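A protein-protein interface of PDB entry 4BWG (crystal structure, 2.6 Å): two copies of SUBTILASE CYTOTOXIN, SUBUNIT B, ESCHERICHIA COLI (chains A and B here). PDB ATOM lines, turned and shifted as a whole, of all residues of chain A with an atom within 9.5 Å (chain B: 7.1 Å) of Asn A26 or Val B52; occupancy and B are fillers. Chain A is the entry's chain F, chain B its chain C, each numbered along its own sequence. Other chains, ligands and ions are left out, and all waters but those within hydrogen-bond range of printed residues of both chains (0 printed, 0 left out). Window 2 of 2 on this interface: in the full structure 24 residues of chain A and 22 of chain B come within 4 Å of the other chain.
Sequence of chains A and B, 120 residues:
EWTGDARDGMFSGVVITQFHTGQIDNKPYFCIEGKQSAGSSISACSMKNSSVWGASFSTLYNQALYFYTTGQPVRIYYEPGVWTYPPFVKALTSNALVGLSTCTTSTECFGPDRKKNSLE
The backbone carbonyl oxygen of Glu B1 sits at hydrogen-bond distance from the backbone NH of Asp A25, 3.0 Å away. The backbone NH (N) of Asn A26 sits at hydrogen-bond distance from the side-chain carboxylate (OE2) of Glu B1 (2.8 Å). The side-chain amide nitrogen (NE2) of Gln A23 lies within hydrogen-bond range of the backbone carbonyl oxygen (O) of Val B52 (2.6 Å). O of Trp B53 sits close to OE1 of Gln A23 (3.3 Å). OE2 of Glu B1 lies within hydrogen-bond range of NE2 of Gln A23. The side-chain hydroxyl (OG) of Ser B56 sits at hydrogen-bond distance from the side-chain amide oxygen (OE1) of Gln A23, at 3.0 Å.
The backbone carbonyl oxygen of Trp B53 sits at hydrogen-bond distance from the side-chain hydroxyl of Ser B56, 2.8 Å away. The backbone NH of Lys A48 is in hydrogen-bond range of the backbone carbonyl oxygen of Pro A28, 2.9 Å away. The indole nitrogen (NE1) of Trp B53 is in hydrogen-bond range of the side-chain carboxylate (OE1) of Glu B79 (2.7 Å).
Ala B55 touches Gln A23. CA of Ile A24 touches O of Glu B1, 3.3 Å away. Asn A26 touches Val B52 (OD1 to O, 3.9 Å). Asn A26 touches Ala B55 (O to CB, 3.4 Å). Pro A28 touches Ala B55 (CG to O, 3.6 Å).
Val B52 touches just these residues of chain A: Gln A23 and Asn A26. No residue of chain A comes within 4 Å of Ser B51. Of the printed residues of chain B, Gln A23 touches Glu B1, Val B52, Trp B53, Ala B55 and Ser B56. Printed residues of chain B within 4 Å of Ile A24: Glu B1 (3.3 Å). Met A47 touches none of the printed residues of chain B. The nearest residue of chain B that does not touch Asn A26 is Ser B51 (5.7 Å). The nearest printed residue of chain B that does not touch Ile A24 is Trp B53 (5.5 Å).
Of the 11 printed residues of chain B, 5 touch a printed residue of chain A. Among the printed residues, no Asp or Glu carboxylate lies within 4 Å of a Lys or Arg side-chain nitrogen of the other chain.
1 position is printed for both chains. Of the 11 pairs that touch across the chains among the printed residues, none has its exchanged pair printed and touching as well.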
ATOM      1  N   GLY A  22     -16.721  -1.975  -2.944  1.00  0.00           N
ATOM      2  CA  GLY A  22     -16.692  -2.811  -4.135  1.00  0.00           C
ATOM      3  C   GLY A  22     -17.739  -2.381  -5.134  1.00  0.00           C
ATOM      4  O   GLY A  22     -18.239  -1.253  -5.067  1.00  0.00           O
ATOM      5  N   GLN A  23     -18.102  -3.296  -6.040  1.00  0.00           N
ATOM      6  CA  GLN A  23     -19.114  -3.093  -7.064  1.00  0.00           C
ATOM      7  C   GLN A  23     -19.893  -4.381  -7.268  1.00  0.00           C
ATOM      8  O   GLN A  23     -19.309  -5.471  -7.233  1.00  0.00           O
ATOM      9  CB  GLN A  23     -18.468  -2.646  -8.385  1.00  0.00           C
ATOM     10  CG  GLN A  23     -19.472  -2.253  -9.466  1.00  0.00           C
ATOM     11  CD  GLN A  23     -18.809  -1.869 -10.750  1.00  0.00           C
ATOM     12  OE1 GLN A  23     -17.964  -0.976 -10.796  1.00  0.00           O
ATOM     13  NE2 GLN A  23     -19.214  -2.513 -11.831  1.00  0.00           N
ATOM     14  N   ILE A  24     -21.213  -4.248  -7.487  1.00  0.00           N
ATOM     15  CA  ILE A  24     -22.105  -5.349  -7.781  1.00  0.00           C
ATOM     16  C   ILE A  24     -23.146  -4.869  -8.780  1.00  0.00           C
ATOM     17  O   ILE A  24     -23.803  -3.851  -8.559  1.00  0.00           O
ATOM     18  CB  ILE A  24     -22.734  -6.011  -6.525  1.00  0.00           C
ATOM     19  CG1 ILE A  24     -23.556  -7.281  -6.925  1.00  0.00           C
ATOM     20  CG2 ILE A  24     -23.549  -5.030  -5.704  1.00  0.00           C
ATOM     21  CD1 ILE A  24     -23.748  -8.289  -5.860  1.00  0.00           C
ATOM     22  N   ASP A  25     -23.261  -5.601  -9.890  1.00  0.00           N
ATOM     23  CA  ASP A  25     -24.205  -5.366 -10.974  1.00  0.00           C
ATOM     24  C   ASP A  25     -24.272  -3.857 -11.372  1.00  0.00           C
ATOM     25  O   ASP A  25     -25.313  -3.192 -11.295  1.00  0.00           O
ATOM     26  CB  ASP A  25     -25.568  -5.966 -10.598  1.00  0.00           C
ATOM     27  CG  ASP A  25     -25.559  -7.503 -10.585  1.00  0.00           C
ATOM     28  OD1 ASP A  25     -25.231  -8.113 -11.642  1.00  0.00           O
ATOM     29  OD2 ASP A  25     -25.844  -8.094  -9.510  1.00  0.00           O
ATOM     30  N   ASN A  26     -23.093  -3.344 -11.766  1.00  0.00           N
ATOM     31  CA  ASN A  26     -22.793  -1.985 -12.233  1.00  0.00           C
ATOM     32  C   ASN A  26     -23.041  -0.880 -11.173  1.00  0.00           C
ATOM     33  O   ASN A  26     -23.016   0.314 -11.506  1.00  0.00           O
ATOM     34  CB  ASN A  26     -23.539  -1.656 -13.520  1.00  0.00           C
ATOM     35  CG  ASN A  26     -22.811  -0.633 -14.358  1.00  0.00           C
ATOM     36  OD1 ASN A  26     -21.633  -0.791 -14.703  1.00  0.00           O
ATOM     37  ND2 ASN A  26     -23.465   0.475 -14.646  1.00  0.00           N
ATOM     38  N   LYS A  27     -23.187  -1.263  -9.900  1.00  0.00           N
ATOM     39  CA  LYS A  27     -23.413  -0.288  -8.856  1.00  0.00           C
ATOM     40  C   LYS A  27     -22.306  -0.330  -7.793  1.00  0.00           C
ATOM     41  O   LYS A  27     -22.147  -1.367  -7.143  1.00  0.00           O
ATOM     42  CB  LYS A  27     -24.792  -0.504  -8.209  1.00  0.00           C
ATOM     43  N   PRO A  28     -21.539   0.776  -7.575  1.00  0.00           N
ATOM     44  CA  PRO A  28     -20.570   0.769  -6.470  1.00  0.00           C
ATOM     45  C   PRO A  28     -21.297   0.723  -5.133  1.00  0.00           C
ATOM     46  O   PRO A  28     -22.418   1.202  -5.024  1.00  0.00           O
ATOM     47  CB  PRO A  28     -19.806   2.087  -6.654  1.00  0.00           C
ATOM     48  CG  PRO A  28     -20.722   2.950  -7.405  1.00  0.00           C
ATOM     49  CD  PRO A  28     -21.582   2.091  -8.247  1.00  0.00           C
ATOM     50  N   TYR A  29     -20.678   0.117  -4.135  1.00  0.00           N
ATOM     51  CA  TYR A  29     -21.234   0.046  -2.770  1.00  0.00           C
ATOM     52  C   TYR A  29     -20.115   0.159  -1.740  1.00  0.00           C
ATOM     53  O   TYR A  29     -18.948  -0.028  -2.076  1.00  0.00           O
ATOM     54  CB  TYR A  29     -22.047  -1.266  -2.534  1.00  0.00           C
ATOM     55  CG  TYR A  29     -21.189  -2.516  -2.490  1.00  0.00           C
ATOM     56  CD1 TYR A  29     -20.872  -3.210  -3.658  1.00  0.00           C
ATOM     57  CD2 TYR A  29     -20.619  -2.954  -1.298  1.00  0.00           C
ATOM     58  CE1 TYR A  29     -20.032  -4.325  -3.633  1.00  0.00           C
ATOM     59  CE2 TYR A  29     -19.753  -4.047  -1.268  1.00  0.00           C
ATOM     60  CZ  TYR A  29     -19.474  -4.738  -2.437  1.00  0.00           C
ATOM     61  OH  TYR A  29     -18.640  -5.831  -2.441  1.00  0.00           O
ATOM     62  N   MET A  47     -25.502   1.247  -1.384  1.00  0.00           N
ATOM     63  CA  MET A  47     -25.256   1.065  -2.827  1.00  0.00           C
ATOM     64  C   MET A  47     -25.707   2.269  -3.615  1.00  0.00           C
ATOM     65  O   MET A  47     -26.809   2.763  -3.383  1.00  0.00           O
ATOM     66  CB  MET A  47     -25.996  -0.157  -3.382  1.00  0.00           C
ATOM     67  CG  MET A  47     -25.495  -1.462  -2.904  1.00  0.00           C
ATOM     68  SD  MET A  47     -26.011  -2.718  -4.080  1.00  0.00           S
ATOM     69  CE  MET A  47     -25.712  -4.190  -3.084  1.00  0.00           C
ATOM     70  N   LYS A  48     -24.907   2.703  -4.579  1.00  0.00           N
ATOM     71  CA  LYS A  48     -25.234   3.841  -5.434  1.00  0.00           C
ATOM     72  C   LYS A  48     -26.333   3.474  -6.400  1.00  0.00           C
ATOM     73  O   LYS A  48     -26.308   2.381  -6.979  1.00  0.00           O
ATOM     74  CB  LYS A  48     -23.994   4.312  -6.207  1.00  0.00           C
ATOM     75  CG  LYS A  48     -24.143   5.653  -6.907  1.00  0.00           C
ATOM     76  CD  LYS A  48     -22.871   5.984  -7.645  1.00  0.00           C
ATOM     77  CE  LYS A  48     -22.913   7.257  -8.440  1.00  0.00           C
ATOM     78  NZ  LYS A  48     -21.553   7.580  -8.950  1.00  0.00           N
ATOM     79  N   ASN A  49     -27.317   4.381  -6.559  1.00  0.00           N
ATOM     80  CA  ASN A  49     -28.466   4.258  -7.473  1.00  0.00           C
ATOM     81  C   ASN A  49     -29.310   2.982  -7.224  1.00  0.00           C
ATOM     82  O   ASN A  49     -30.040   2.552  -8.110  1.00  0.00           O
ATOM     83  CB  ASN A  49     -28.005   4.323  -8.947  1.00  0.00           C
ATOM     84  CG  ASN A  49     -27.217   5.568  -9.314  1.00  0.00           C
ATOM     85  OD1 ASN A  49     -27.527   6.688  -8.886  1.00  0.00           O
ATOM     86  ND2 ASN A  49     -26.188   5.401 -10.137  1.00  0.00           N
ATOM     87  N   SER A  50     -29.223   2.397  -6.020  1.00  0.00           N
ATOM     88  CA  SER A  50     -30.021   1.237  -5.644  1.00  0.00           C
ATOM     89  C   SER A  50     -31.016   1.654  -4.594  1.00  0.00           C
ATOM     90  O   SER A  50     -30.701   1.685  -3.392  1.00  0.00           O
ATOM     91  CB  SER A  50     -29.162   0.069  -5.177  1.00  0.00           C
ATOM     92  OG  SER A  50     -28.755  -0.682  -6.310  1.00  0.00           O
ATOM     93  N   GLU B   1     -21.859  -9.087 -12.200  1.00  0.00           N
ATOM     94  CA  GLU B   1     -20.505  -9.085 -11.655  1.00  0.00           C
ATOM     95  C   GLU B   1     -20.528  -8.632 -10.195  1.00  0.00           C
ATOM     96  O   GLU B   1     -21.428  -7.913  -9.767  1.00  0.00           O
ATOM     97  CB  GLU B   1     -19.545  -8.209 -12.515  1.00  0.00           C
ATOM     98  CG  GLU B   1     -19.422  -6.733 -12.132  1.00  0.00           C
ATOM     99  CD  GLU B   1     -20.676  -5.883 -12.247  1.00  0.00           C
ATOM    100  OE1 GLU B   1     -21.631  -6.320 -12.930  1.00  0.00           O
ATOM    101  OE2 GLU B   1     -20.697  -4.770 -11.665  1.00  0.00           O
ATOM    102  N   SER B  50     -14.828   2.664 -18.067  1.00  0.00           N
ATOM    103  CA  SER B  50     -14.320   1.461 -18.733  1.00  0.00           C
ATOM    104  C   SER B  50     -14.866   0.267 -18.007  1.00  0.00           C
ATOM    105  O   SER B  50     -14.291  -0.176 -17.003  1.00  0.00           O
ATOM    106  CB  SER B  50     -12.795   1.432 -18.777  1.00  0.00           C
ATOM    107  OG  SER B  50     -12.349   2.237 -19.855  1.00  0.00           O
ATOM    108  N   SER B  51     -16.034  -0.199 -18.495  1.00  0.00           N
ATOM    109  CA  SER B  51     -16.814  -1.346 -18.036  1.00  0.00           C
ATOM    110  C   SER B  51     -15.898  -2.584 -17.896  1.00  0.00           C
ATOM    111  O   SER B  51     -14.840  -2.632 -18.529  1.00  0.00           O
ATOM    112  CB  SER B  51     -17.970  -1.599 -19.009  1.00  0.00           C
ATOM    113  N   VAL B  52     -16.235  -3.566 -17.054  1.00  0.00           N
ATOM    114  CA  VAL B  52     -17.417  -3.720 -16.202  1.00  0.00           C
ATOM    115  C   VAL B  52     -17.240  -2.953 -14.898  1.00  0.00           C
ATOM    116  O   VAL B  52     -18.224  -2.697 -14.208  1.00  0.00           O
ATOM    117  CB  VAL B  52     -17.636  -5.227 -15.883  1.00  0.00           C
ATOM    118  CG1 VAL B  52     -19.097  -5.520 -15.576  1.00  0.00           C
ATOM    119  CG2 VAL B  52     -17.117  -6.128 -16.997  1.00  0.00           C
ATOM    120  N   TRP B  53     -15.985  -2.629 -14.535  1.00  0.00           N
ATOM    121  CA  TRP B  53     -15.639  -2.018 -13.250  1.00  0.00           C
ATOM    122  C   TRP B  53     -15.524  -0.485 -13.269  1.00  0.00           C
ATOM    123  O   TRP B  53     -15.193   0.087 -12.238  1.00  0.00           O
ATOM    124  CB  TRP B  53     -14.337  -2.654 -12.742  1.00  0.00           C
ATOM    125  CG  TRP B  53     -14.400  -4.157 -12.723  1.00  0.00           C
ATOM    126  CD1 TRP B  53     -13.801  -5.013 -13.601  1.00  0.00           C
ATOM    127  CD2 TRP B  53     -15.168  -4.976 -11.824  1.00  0.00           C
ATOM    128  NE1 TRP B  53     -14.106  -6.318 -13.275  1.00  0.00           N
ATOM    129  CE2 TRP B  53     -14.951  -6.322 -12.193  1.00  0.00           C
ATOM    130  CE3 TRP B  53     -15.982  -4.705 -10.707  1.00  0.00           C
ATOM    131  CZ2 TRP B  53     -15.508  -7.389 -11.483  1.00  0.00           C
ATOM    132  CZ3 TRP B  53     -16.559  -5.765 -10.028  1.00  0.00           C
ATOM    133  CH2 TRP B  53     -16.308  -7.086 -10.406  1.00  0.00           C
ATOM    134  N   GLY B  54     -15.869   0.152 -14.389  1.00  0.00           N
ATOM    135  CA  GLY B  54     -15.821   1.604 -14.578  1.00  0.00           C
ATOM    136  C   GLY B  54     -16.632   2.462 -13.615  1.00  0.00           C
ATOM    137  O   GLY B  54     -16.225   3.581 -13.285  1.00  0.00           O
ATOM    138  N   ALA B  55     -17.777   1.934 -13.143  1.00  0.00           N
ATOM    139  CA  ALA B  55     -18.714   2.597 -12.236  1.00  0.00           C
ATOM    140  C   ALA B  55     -18.115   2.851 -10.850  1.00  0.00           C
ATOM    141  O   ALA B  55     -18.562   3.763 -10.153  1.00  0.00           O
ATOM    142  CB  ALA B  55     -19.994   1.775 -12.106  1.00  0.00           C
ATOM    143  N   SER B  56     -17.101   2.072 -10.452  1.00  0.00           N
ATOM    144  CA  SER B  56     -16.478   2.188  -9.131  1.00  0.00           C
ATOM    145  C   SER B  56     -15.189   3.029  -9.130  1.00  0.00           C
ATOM    146  O   SER B  56     -14.579   3.179  -8.087  1.00  0.00           O
ATOM    147  CB  SER B  56     -16.214   0.804  -8.555  1.00  0.00           C
ATOM    148  OG  SER B  56     -15.445   0.042  -9.463  1.00  0.00           O
ATOM    149  N   GLU B  79      -9.132  -8.114 -10.813  1.00  0.00           N
ATOM    150  CA  GLU B  79      -9.519  -9.026 -11.858  1.00  0.00           C
ATOM    151  C   GLU B  79      -8.433  -9.025 -12.922  1.00  0.00           C
ATOM    152  O   GLU B  79      -8.213  -7.988 -13.560  1.00  0.00           O
ATOM    153  CB  GLU B  79     -10.884  -8.709 -12.456  1.00  0.00           C
ATOM    154  CG  GLU B  79     -11.368  -9.864 -13.306  1.00  0.00           C
ATOM    155  CD  GLU B  79     -12.367  -9.584 -14.398  1.00  0.00           C
ATOM    156  OE1 GLU B  79     -13.270  -8.741 -14.205  1.00  0.00           O
ATOM    157  OE2 GLU B  79     -12.221 -10.199 -15.478  1.00  0.00           O
ATOM    158  N   VAL B  82      -8.104  -7.695 -17.602  1.00  0.00           N
ATOM    159  CA  VAL B  82      -9.133  -6.731 -17.967  1.00  0.00           C
ATOM    160  C   VAL B  82      -8.588  -5.730 -19.002  1.00  0.00           C
ATOM    161  O   VAL B  82      -9.244  -5.516 -20.023  1.00  0.00           O
ATOM    162  CB  VAL B  82      -9.743  -6.055 -16.724  1.00  0.00           C
ATOM    163  CG1 VAL B  82     -10.750  -4.980 -17.097  1.00  0.00           C
ATOM    164  CG2 VAL B  82     -10.413  -7.095 -15.846  1.00  0.00           C
ATOM    165  N   TRP B  83      -7.398  -5.149 -18.772  1.00  0.00           N
ATOM    166  CA  TRP B  83      -6.805  -4.180 -19.711  1.00  0.00           C
ATOM    167  C   TRP B  83      -6.069  -4.929 -20.798  1.00  0.00           C
ATOM    168  O   TRP B  83      -5.448  -5.961 -20.523  1.00  0.00           O
ATOM    169  CB  TRP B  83      -5.928  -3.166 -18.983  1.00  0.00           C
ATOM    170  CG  TRP B  83      -6.580  -2.689 -17.711  1.00  0.00           C
ATOM    171  CD1 TRP B  83      -6.115  -2.844 -16.440  1.00  0.00           C
ATOM    172  CD2 TRP B  83      -7.864  -2.061 -17.594  1.00  0.00           C
ATOM    173  NE1 TRP B  83      -7.006  -2.318 -15.544  1.00  0.00           N
ATOM    174  CE2 TRP B  83      -8.101  -1.851 -16.223  1.00  0.00           C
ATOM    175  CE3 TRP B  83      -8.843  -1.654 -18.522  1.00  0.00           C
ATOM    176  CZ2 TRP B  83      -9.270  -1.252 -15.757  1.00  0.00           C
ATOM    177  CZ3 TRP B  83      -9.989  -1.048 -18.060  1.00  0.00           C
ATOM    178  CH2 TRP B  83     -10.204  -0.876 -16.692  1.00  0.00           C
